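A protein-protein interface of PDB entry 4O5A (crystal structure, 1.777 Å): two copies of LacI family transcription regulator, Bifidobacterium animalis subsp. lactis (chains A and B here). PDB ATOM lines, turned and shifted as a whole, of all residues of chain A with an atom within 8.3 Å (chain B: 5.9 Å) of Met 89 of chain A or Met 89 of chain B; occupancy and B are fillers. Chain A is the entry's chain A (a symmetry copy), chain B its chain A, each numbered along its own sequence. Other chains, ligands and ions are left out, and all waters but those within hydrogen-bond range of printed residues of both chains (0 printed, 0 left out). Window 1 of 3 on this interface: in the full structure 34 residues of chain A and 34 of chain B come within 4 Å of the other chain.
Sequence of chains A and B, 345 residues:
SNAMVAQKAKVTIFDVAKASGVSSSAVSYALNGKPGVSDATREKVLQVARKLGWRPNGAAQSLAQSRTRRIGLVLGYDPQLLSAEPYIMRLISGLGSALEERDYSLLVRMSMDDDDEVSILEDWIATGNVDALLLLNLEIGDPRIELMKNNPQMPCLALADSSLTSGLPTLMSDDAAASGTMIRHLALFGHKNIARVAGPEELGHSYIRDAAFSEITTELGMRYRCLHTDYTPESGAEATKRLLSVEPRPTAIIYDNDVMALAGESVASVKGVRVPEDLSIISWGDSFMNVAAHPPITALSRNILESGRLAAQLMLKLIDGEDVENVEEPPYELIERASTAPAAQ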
ATOM      1  N   LEU A  73      16.170 -21.107   9.639  1.00  0.00           N
ATOM      2  CA  LEU A  73      14.988 -21.064   8.786  1.00  0.00           C
ATOM      3  C   LEU A  73      15.383 -20.576   7.415  1.00  0.00           C
ATOM      4  O   LEU A  73      15.923 -19.475   7.274  1.00  0.00           O
ATOM      5  CB  LEU A  73      13.923 -20.128   9.380  1.00  0.00           C
ATOM      6  CG  LEU A  73      12.693 -19.867   8.508  1.00  0.00           C
ATOM      7  CD1 LEU A  73      11.979 -21.171   8.184  1.00  0.00           C
ATOM      8  CD2 LEU A  73      11.755 -18.917   9.218  1.00  0.00           C
ATOM      9  N   LEU A  75      13.896 -19.251   4.012  1.00  0.00           N
ATOM     10  CA  LEU A  75      12.681 -18.757   3.363  1.00  0.00           C
ATOM     11  C   LEU A  75      12.837 -18.755   1.849  1.00  0.00           C
ATOM     12  O   LEU A  75      13.957 -18.738   1.331  1.00  0.00           O
ATOM     13  CB  LEU A  75      12.350 -17.346   3.845  1.00  0.00           C
ATOM     14  CG  LEU A  75      12.012 -17.190   5.323  1.00  0.00           C
ATOM     15  CD1 LEU A  75      11.812 -15.720   5.669  1.00  0.00           C
ATOM     16  CD2 LEU A  75      10.769 -17.988   5.639  1.00  0.00           C
ATOM     17  N   GLY A  76      11.719 -18.763   1.129  1.00  0.00           N
ATOM     18  CA  GLY A  76      11.780 -18.700  -0.321  1.00  0.00           C
ATOM     19  C   GLY A  76      11.711 -17.261  -0.788  1.00  0.00           C
ATOM     20  O   GLY A  76      10.951 -16.468  -0.231  1.00  0.00           O
ATOM     21  N   TYR A  77      12.502 -16.910  -1.797  1.00  0.00           N
ATOM     22  CA  TYR A  77      12.497 -15.544  -2.314  1.00  0.00           C
ATOM     23  C   TYR A  77      11.139 -15.208  -2.930  1.00  0.00           C
ATOM     24  O   TYR A  77      10.614 -15.971  -3.747  1.00  0.00           O
ATOM     25  CB  TYR A  77      13.610 -15.339  -3.341  1.00  0.00           C
ATOM     26  CG  TYR A  77      13.653 -13.940  -3.920  1.00  0.00           C
ATOM     27  CD1 TYR A  77      14.074 -12.861  -3.150  1.00  0.00           C
ATOM     28  CD2 TYR A  77      13.276 -13.698  -5.231  1.00  0.00           C
ATOM     29  CE1 TYR A  77      14.119 -11.579  -3.676  1.00  0.00           C
ATOM     30  CE2 TYR A  77      13.313 -12.421  -5.763  1.00  0.00           C
ATOM     31  CZ  TYR A  77      13.737 -11.367  -4.980  1.00  0.00           C
ATOM     32  OH  TYR A  77      13.777 -10.096  -5.511  1.00  0.00           O
ATOM     33  N   ASP A  78      10.598 -14.055  -2.532  1.00  0.00           N
ATOM     34  CA  ASP A  78       9.232 -13.633  -2.857  1.00  0.00           C
ATOM     35  C   ASP A  78       8.194 -14.587  -2.285  1.00  0.00           C
ATOM     36  O   ASP A  78       8.099 -14.746  -1.068  1.00  0.00           O
ATOM     37  CB  ASP A  78       9.027 -13.453  -4.362  1.00  0.00           C
ATOM     38  CG  ASP A  78       9.528 -12.122  -4.855  1.00  0.00           C
ATOM     39  OD1 ASP A  78       9.697 -11.214  -4.014  1.00  0.00           O
ATOM     40  OD2 ASP A  78       9.743 -11.982  -6.078  1.00  0.00           O
ATOM     41  N   TYR A  87       1.467 -14.540   6.582  1.00  0.00           N
ATOM     42  CA  TYR A  87       1.562 -15.752   7.376  1.00  0.00           C
ATOM     43  C   TYR A  87       2.919 -15.886   8.053  1.00  0.00           C
ATOM     44  O   TYR A  87       3.015 -16.081   9.271  1.00  0.00           O
ATOM     45  CB  TYR A  87       1.323 -16.979   6.497  1.00  0.00           C
ATOM     46  CG  TYR A  87       1.719 -18.271   7.178  1.00  0.00           C
ATOM     47  CD1 TYR A  87       0.910 -18.836   8.147  1.00  0.00           C
ATOM     48  CD2 TYR A  87       2.905 -18.923   6.856  1.00  0.00           C
ATOM     49  CE1 TYR A  87       1.266 -20.010   8.780  1.00  0.00           C
ATOM     50  CE2 TYR A  87       3.268 -20.104   7.487  1.00  0.00           C
ATOM     51  CZ  TYR A  87       2.441 -20.642   8.447  1.00  0.00           C
ATOM     52  OH  TYR A  87       2.787 -21.815   9.079  1.00  0.00           O
ATOM     53  N   ILE A  88       3.972 -15.833   7.247  1.00  0.00           N
ATOM     54  CA  ILE A  88       5.321 -16.029   7.752  1.00  0.00           C
ATOM     55  C   ILE A  88       5.657 -14.991   8.815  1.00  0.00           C
ATOM     56  O   ILE A  88       6.310 -15.325   9.806  1.00  0.00           O
ATOM     57  CB  ILE A  88       6.375 -15.992   6.619  1.00  0.00           C
ATOM     58  CG1 ILE A  88       6.186 -17.183   5.680  1.00  0.00           C
ATOM     59  CG2 ILE A  88       7.785 -16.042   7.187  1.00  0.00           C
ATOM     60  CD1 ILE A  88       6.536 -18.519   6.316  1.00  0.00           C
ATOM     61  N   MET A  89       5.202 -13.748   8.631  1.00  0.00           N
ATOM     62  CA  MET A  89       5.521 -12.725   9.637  1.00  0.00           C
ATOM     63  C   MET A  89       4.912 -13.094  10.983  1.00  0.00           C
ATOM     64  O   MET A  89       5.547 -12.960  12.018  1.00  0.00           O
ATOM     65  CB  MET A  89       5.059 -11.325   9.213  1.00  0.00           C
ATOM     66  CG  MET A  89       6.112 -10.488   8.516  1.00  0.00           C
ATOM     67  SD  MET A  89       7.951 -10.746   9.121  1.00  0.00           S
ATOM     68  CE  MET A  89       7.855  -9.650  10.738  1.00  0.00           C
ATOM     69  N   ARG A  90       3.681 -13.583  10.968  1.00  0.00           N
ATOM     70  CA  ARG A  90       3.039 -13.967  12.223  1.00  0.00           C
ATOM     71  C   ARG A  90       3.731 -15.157  12.839  1.00  0.00           C
ATOM     72  O   ARG A  90       3.875 -15.231  14.060  1.00  0.00           O
ATOM     73  CB  ARG A  90       1.569 -14.301  12.010  1.00  0.00           C
ATOM     74  CG  ARG A  90       0.676 -13.115  11.799  1.00  0.00           C
ATOM     75  CD  ARG A  90      -0.729 -13.588  11.496  1.00  0.00           C
ATOM     76  NE  ARG A  90      -1.363 -12.718  10.522  1.00  0.00           N
ATOM     77  CZ  ARG A  90      -2.450 -13.027   9.821  1.00  0.00           C
ATOM     78  NH1 ARG A  90      -3.043 -14.201   9.975  1.00  0.00           N
ATOM     79  NH2 ARG A  90      -2.939 -12.152   8.961  1.00  0.00           N
ATOM     80  N   LEU A  91       4.149 -16.106  12.006  1.00  0.00           N
ATOM     81  CA  LEU A  91       4.884 -17.262  12.511  1.00  0.00           C
ATOM     82  C   LEU A  91       6.171 -16.823  13.189  1.00  0.00           C
ATOM     83  O   LEU A  91       6.523 -17.314  14.271  1.00  0.00           O
ATOM     84  CB  LEU A  91       5.208 -18.233  11.371  1.00  0.00           C
ATOM     85  CG  LEU A  91       5.642 -19.615  11.860  1.00  0.00           C
ATOM     86  CD1 LEU A  91       4.432 -20.357  12.429  1.00  0.00           C
ATOM     87  CD2 LEU A  91       6.300 -20.413  10.745  1.00  0.00           C
ATOM     88  N   ILE A  92       6.881 -15.902  12.550  1.00  0.00           N
ATOM     89  CA  ILE A  92       8.148 -15.433  13.096  1.00  0.00           C
ATOM     90  C   ILE A  92       7.953 -14.688  14.424  1.00  0.00           C
ATOM     91  O   ILE A  92       8.784 -14.824  15.336  1.00  0.00           O
ATOM     92  CB  ILE A  92       8.923 -14.585  12.056  1.00  0.00           C
ATOM     93  CG1 ILE A  92       9.463 -15.510  10.964  1.00  0.00           C
ATOM     94  CG2 ILE A  92      10.077 -13.835  12.698  1.00  0.00           C
ATOM     95  CD1 ILE A  92      10.149 -14.779   9.834  1.00  0.00           C
ATOM     96  N   SER A  93       6.882 -13.908  14.538  1.00  0.00           N
ATOM     97  CA  SER A  93       6.528 -13.275  15.815  1.00  0.00           C
ATOM     98  C   SER A  93       6.278 -14.303  16.929  1.00  0.00           C
ATOM     99  O   SER A  93       6.749 -14.133  18.055  1.00  0.00           O
ATOM    100  CB  SER A  93       5.301 -12.378  15.672  1.00  0.00           C
ATOM    101  OG  SER A  93       5.629 -11.196  14.978  1.00  0.00           O
ATOM    102  N   GLY A  94       5.522 -15.351  16.619  1.00  0.00           N
ATOM    103  CA  GLY A  94       5.272 -16.409  17.582  1.00  0.00           C
ATOM    104  C   GLY A  94       6.549 -17.144  17.953  1.00  0.00           C
ATOM    105  O   GLY A  94       6.808 -17.405  19.140  1.00  0.00           O
ATOM    106  N   LEU A  95       7.350 -17.505  16.952  1.00  0.00           N
ATOM    107  CA  LEU A  95       8.629 -18.158  17.224  1.00  0.00           C
ATOM    108  C   LEU A  95       9.461 -17.302  18.172  1.00  0.00           C
ATOM    109  O   LEU A  95       9.942 -17.785  19.198  1.00  0.00           O
ATOM    110  CB  LEU A  95       9.432 -18.366  15.927  1.00  0.00           C
ATOM    111  CG  LEU A  95       9.049 -19.512  14.988  1.00  0.00           C
ATOM    112  CD1 LEU A  95       9.608 -19.240  13.593  1.00  0.00           C
ATOM    113  CD2 LEU A  95       9.580 -20.850  15.503  1.00  0.00           C
ATOM    114  N   GLY A  96       9.611 -16.027  17.833  1.00  0.00           N
ATOM    115  CA  GLY A  96      10.385 -15.111  18.648  1.00  0.00           C
ATOM    116  C   GLY A  96       9.892 -14.978  20.076  1.00  0.00           C
ATOM    117  O   GLY A  96      10.701 -14.810  20.987  1.00  0.00           O
ATOM    118  N   VAL A 108      18.120 -16.549   9.486  1.00  0.00           N
ATOM    119  CA  VAL A 108      17.302 -16.594   8.279  1.00  0.00           C
ATOM    120  C   VAL A 108      18.150 -16.500   7.029  1.00  0.00           C
ATOM    121  O   VAL A 108      18.950 -15.568   6.868  1.00  0.00           O
ATOM    122  CB  VAL A 108      16.275 -15.460   8.267  1.00  0.00           C
ATOM    123  CG1 VAL A 108      15.483 -15.460   6.948  1.00  0.00           C
ATOM    124  CG2 VAL A 108      15.339 -15.586   9.451  1.00  0.00           C
ATOM    125  N   MET A 110      17.831 -17.242   2.513  1.00  0.00           N
ATOM    126  CA  MET A 110      16.834 -17.084   1.463  1.00  0.00           C
ATOM    127  C   MET A 110      17.228 -17.976   0.300  1.00  0.00           C
ATOM    128  O   MET A 110      18.324 -17.840  -0.245  1.00  0.00           O
ATOM    129  CB  MET A 110      16.789 -15.605   1.029  1.00  0.00           C
ATOM    130  CG  MET A 110      15.640 -15.172   0.098  1.00  0.00           C
ATOM    131  SD  MET A 110      13.905 -14.947   0.983  1.00  0.00           S
ATOM    132  CE  MET A 110      14.499 -14.229   2.681  1.00  0.00           C
ATOM    133  N   ILE A 304      -1.787 -18.673  14.030  1.00  0.00           N
ATOM    134  CA  ILE A 304      -0.400 -18.719  13.581  1.00  0.00           C
ATOM    135  C   ILE A 304       0.585 -18.265  14.647  1.00  0.00           C
ATOM    136  O   ILE A 304       1.683 -18.810  14.751  1.00  0.00           O
ATOM    137  CB  ILE A 304      -0.204 -17.846  12.344  1.00  0.00           C
ATOM    138  CG1 ILE A 304      -1.197 -18.267  11.259  1.00  0.00           C
ATOM    139  CG2 ILE A 304       1.228 -17.977  11.830  1.00  0.00           C
ATOM    140  CD1 ILE A 304      -1.381 -17.212  10.169  1.00  0.00           C
ATOM    141  N   LEU A 305       0.207 -17.249  15.420  1.00  0.00           N
ATOM    142  CA  LEU A 305       1.053 -16.789  16.522  1.00  0.00           C
ATOM    143  C   LEU A 305       1.363 -17.932  17.477  1.00  0.00           C
ATOM    144  O   LEU A 305       2.533 -18.230  17.735  1.00  0.00           O
ATOM    145  CB  LEU A 305       0.389 -15.649  17.291  1.00  0.00           C
ATOM    146  CG  LEU A 305       0.518 -14.229  16.745  1.00  0.00           C
ATOM    147  CD1 LEU A 305      -0.351 -13.287  17.568  1.00  0.00           C
ATOM    148  CD2 LEU A 305       1.977 -13.801  16.805  1.00  0.00           C
ATOM    149  N   LEU B  75      13.220  -7.200  15.437  1.00  0.00           N
ATOM    150  CA  LEU B  75      11.847  -6.865  15.059  1.00  0.00           C
ATOM    151  C   LEU B  75      10.983  -6.642  16.292  1.00  0.00           C
ATOM    152  O   LEU B  75      11.306  -7.120  17.383  1.00  0.00           O
ATOM    153  CB  LEU B  75      11.239  -7.976  14.204  1.00  0.00           C
ATOM    154  CG  LEU B  75      11.892  -8.234  12.851  1.00  0.00           C
ATOM    155  CD1 LEU B  75      11.246  -9.432  12.169  1.00  0.00           C
ATOM    156  CD2 LEU B  75      11.766  -6.997  11.992  1.00  0.00           C
ATOM    157  N   TYR B  87       5.143  -5.349   4.732  1.00  0.00           N
ATOM    158  CA  TYR B  87       6.314  -4.542   4.439  1.00  0.00           C
ATOM    159  C   TYR B  87       7.607  -5.256   4.813  1.00  0.00           C
ATOM    160  O   TYR B  87       8.530  -5.386   4.000  1.00  0.00           O
ATOM    161  CB  TYR B  87       6.244  -3.216   5.196  1.00  0.00           C
ATOM    162  CG  TYR B  87       7.562  -2.472   5.196  1.00  0.00           C
ATOM    163  CD1 TYR B  87       7.985  -1.783   4.073  1.00  0.00           C
ATOM    164  CD2 TYR B  87       8.388  -2.464   6.315  1.00  0.00           C
ATOM    165  CE1 TYR B  87       9.189  -1.109   4.058  1.00  0.00           C
ATOM    166  CE2 TYR B  87       9.598  -1.787   6.308  1.00  0.00           C
ATOM    167  CZ  TYR B  87       9.991  -1.109   5.176  1.00  0.00           C
ATOM    168  OH  TYR B  87      11.188  -0.431   5.156  1.00  0.00           O
ATOM    169  N   ILE B  88       7.690  -5.672   6.071  1.00  0.00           N
ATOM    170  CA  ILE B  88       8.901  -6.296   6.581  1.00  0.00           C
ATOM    171  C   ILE B  88       9.241  -7.550   5.786  1.00  0.00           C
ATOM    172  O   ILE B  88      10.418  -7.802   5.521  1.00  0.00           O
ATOM    173  CB  ILE B  88       8.788  -6.634   8.087  1.00  0.00           C
ATOM    174  CG1 ILE B  88       8.690  -5.351   8.913  1.00  0.00           C
ATOM    175  CG2 ILE B  88       9.999  -7.423   8.560  1.00  0.00           C
ATOM    176  CD1 ILE B  88       9.975  -4.538   8.925  1.00  0.00           C
ATOM    177  N   MET B  89       8.226  -8.323   5.387  1.00  0.00           N
ATOM    178  CA  MET B  89       8.527  -9.544   4.627  1.00  0.00           C
ATOM    179  C   MET B  89       9.204  -9.197   3.308  1.00  0.00           C
ATOM    180  O   MET B  89      10.161  -9.840   2.905  1.00  0.00           O
ATOM    181  CB  MET B  89       7.277 -10.396   4.372  1.00  0.00           C
ATOM    182  CG  MET B  89       7.031 -11.491   5.389  1.00  0.00           C
ATOM    183  SD  MET B  89       8.624 -12.332   6.145  1.00  0.00           S
ATOM    184  CE  MET B  89       9.029 -13.527   4.651  1.00  0.00           C
ATOM    185  N   ARG B  90       8.720  -8.159   2.643  1.00  0.00           N
ATOM    186  CA  ARG B  90       9.328  -7.764   1.375  1.00  0.00           C
ATOM    187  C   ARG B  90      10.727  -7.243   1.587  1.00  0.00           C
ATOM    188  O   ARG B  90      11.619  -7.500   0.777  1.00  0.00           O
ATOM    189  CB  ARG B  90       8.500  -6.694   0.676  1.00  0.00           C
ATOM    190  CG  ARG B  90       7.239  -7.191   0.032  1.00  0.00           C
ATOM    191  CD  ARG B  90       6.465  -6.020  -0.530  1.00  0.00           C
ATOM    192  NE  ARG B  90       5.036  -6.230  -0.374  1.00  0.00           N
ATOM    193  CZ  ARG B  90       4.113  -5.278  -0.471  1.00  0.00           C
ATOM    194  NH1 ARG B  90       4.458  -4.025  -0.723  1.00  0.00           N
ATOM    195  NH2 ARG B  90       2.839  -5.589  -0.310  1.00  0.00           N
ATOM    196  N   LEU B  91      10.931  -6.494   2.667  1.00  0.00           N
ATOM    197  CA  LEU B  91      12.268  -6.000   2.985  1.00  0.00           C
ATOM    198  C   LEU B  91      13.228  -7.158   3.198  1.00  0.00           C
ATOM    199  O   LEU B  91      14.366  -7.144   2.707  1.00  0.00           O
ATOM    200  CB  LEU B  91      12.234  -5.122   4.239  1.00  0.00           C
ATOM    201  CG  LEU B  91      13.499  -4.283   4.424  1.00  0.00           C
ATOM    202  CD1 LEU B  91      13.523  -3.162   3.385  1.00  0.00           C
ATOM    203  CD2 LEU B  91      13.589  -3.725   5.837  1.00  0.00           C
ATOM    204  N   ILE B  92      12.775  -8.162   3.939  1.00  0.00           N
ATOM    205  CA  ILE B  92      13.624  -9.309   4.233  1.00  0.00           C
ATOM    206  C   ILE B  92      13.969 -10.101   2.964  1.00  0.00           C
ATOM    207  O   ILE B  92      15.100 -10.593   2.831  1.00  0.00           O
ATOM    208  CB  ILE B  92      12.994 -10.202   5.330  1.00  0.00           C
ATOM    209  CG1 ILE B  92      13.093  -9.482   6.676  1.00  0.00           C
ATOM    210  CG2 ILE B  92      13.695 -11.546   5.424  1.00  0.00           C
ATOM    211  CD1 ILE B  92      12.413 -10.215   7.808  1.00  0.00           C
ATOM    212  N   SER B  93      13.014 -10.232   2.046  1.00  0.00           N
ATOM    213  CA  SER B  93      13.288 -10.840   0.738  1.00  0.00           C
ATOM    214  C   SER B  93      14.366 -10.077  -0.048  1.00  0.00           C
ATOM    215  O   SER B  93      15.266 -10.686  -0.630  1.00  0.00           O
ATOM    216  CB  SER B  93      12.022 -10.939  -0.109  1.00  0.00           C
ATOM    217  OG  SER B  93      11.177 -11.956   0.380  1.00  0.00           O
ATOM    218  N   GLY B  94      14.259  -8.753  -0.081  1.00  0.00           N
ATOM    219  CA  GLY B  94      15.257  -7.934  -0.747  1.00  0.00           C
ATOM    220  C   GLY B  94      16.613  -8.042  -0.073  1.00  0.00           C
ATOM    221  O   GLY B  94      17.646  -8.194  -0.748  1.00  0.00           O
ATOM    222  N   MET B 110      13.567 -10.580  18.635  1.00  0.00           N
ATOM    223  CA  MET B 110      12.240  -9.994  18.762  1.00  0.00           C
ATOM    224  C   MET B 110      12.192  -9.213  20.063  1.00  0.00           C
ATOM    225  O   MET B 110      12.424  -9.773  21.134  1.00  0.00           O
ATOM    226  CB  MET B 110      11.189 -11.122  18.762  1.00  0.00           C
ATOM    227  CG  MET B 110       9.707 -10.713  18.648  1.00  0.00           C
ATOM    228  SD  MET B 110       9.131 -10.199  16.847  1.00  0.00           S
ATOM    229  CE  MET B 110      10.185 -11.444  15.802  1.00  0.00           C
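SD of Met 89 of chain B lies close to SD of Met 89 of chain A (3.4 Å).
The backbone carbonyl oxygen (O) of Met 89 of chain B lies within hydrogen-bond range of the side-chain hydroxyl (OG) of Ser 93 of chain B. N of Tyr 77 of chain A lies close to SD of Met 110 of chain A (3.7 Å). The backbone carbonyl oxygen (O) of Met 89 of chain A lies within hydrogen-bond range of the side-chain hydroxyl (OG) of Ser 93 of chain A (3.4 Å).
Among the printed residues, merely in contact across the chains: Tyr 77 of chain A with Ser 93 of chain B (3.4 Å), Asp 78 of chain A with Ser 93 of chain B (3.6 Å), Leu 75 of chain A with Met 89 of chain B (3.7 Å), Met 89 of chain A with Leu 75 of chain B (3.7 Å), Met 110 of chain A with Ile 92 of chain B (3.7 Å), Ile 92 of chain A with Met 110 of chain B (3.7 Å), Met 89 of chain A with Ile 88 of chain B (3.8 Å) and Ile 88 of chain A with Met 89 of chain B (3.8 Å).
Met 89 of chain A touches just these residues of chain B: Leu 75, Ile 88 and Met 89. Met 89 of chain B touches just these residues of chain A: Leu 75, Ile 88 and Met 89. Printed residues of chain A within 4 Å of Ile 88 of chain B: Met 89 (3.8 Å). Of the printed residues of chain A, Ile 92 of chain B touches Met 110. Printed residues of chain A within 4 Å of Ser 93 of chain B: Tyr 77 (3.4 Å) and Asp 78 (3.6 Å). Of the printed residues of chain B, Tyr 77 of chain A touches Ser 93 (3.4 Å). Printed residues of chain B within 4 Å of Ile 92 of chain A: Met 110 (3.7 Å). The nearest residue of chain A that does not touch Met 89 of chain B is Ile 92 of chain A (4.7 Å).
Of the 10 printed residues of chain B, 6 touch a printed residue of chain A. Hydrophobic or aromatic side chains of chain B within 4 Å of the printed part of chain A: Leu 75, Ile 88, Met 89, Ile 92 and Met 110. Among the printed residues, 9 pairs touch across the chains. Among the printed residues, no Asp or Glu carboxylate lies within 4 Å of a Lys or Arg side-chain nitrogen of the other chain.
Leu 75 of chain A touches Met 89 of chain B, and with the chains exchanged Met 89 of chain A touches Leu 75 of chain B. Ile 88 of chain A touches Met 89 of chain B, and with the chains exchanged Met 89 of chain A touches Ile 88 of chain B. Met 89 of chain B touches its own counterpart, Met 89 of chain A. Ile 92 of chain A touches Met 110 of chain B, and with the chains exchanged Met 110 of chain A touches Ile 92 of chain B. Positions printed for both chains: 75, 87, 88, 89, 90, 91, 92, 93, 94 and 110.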
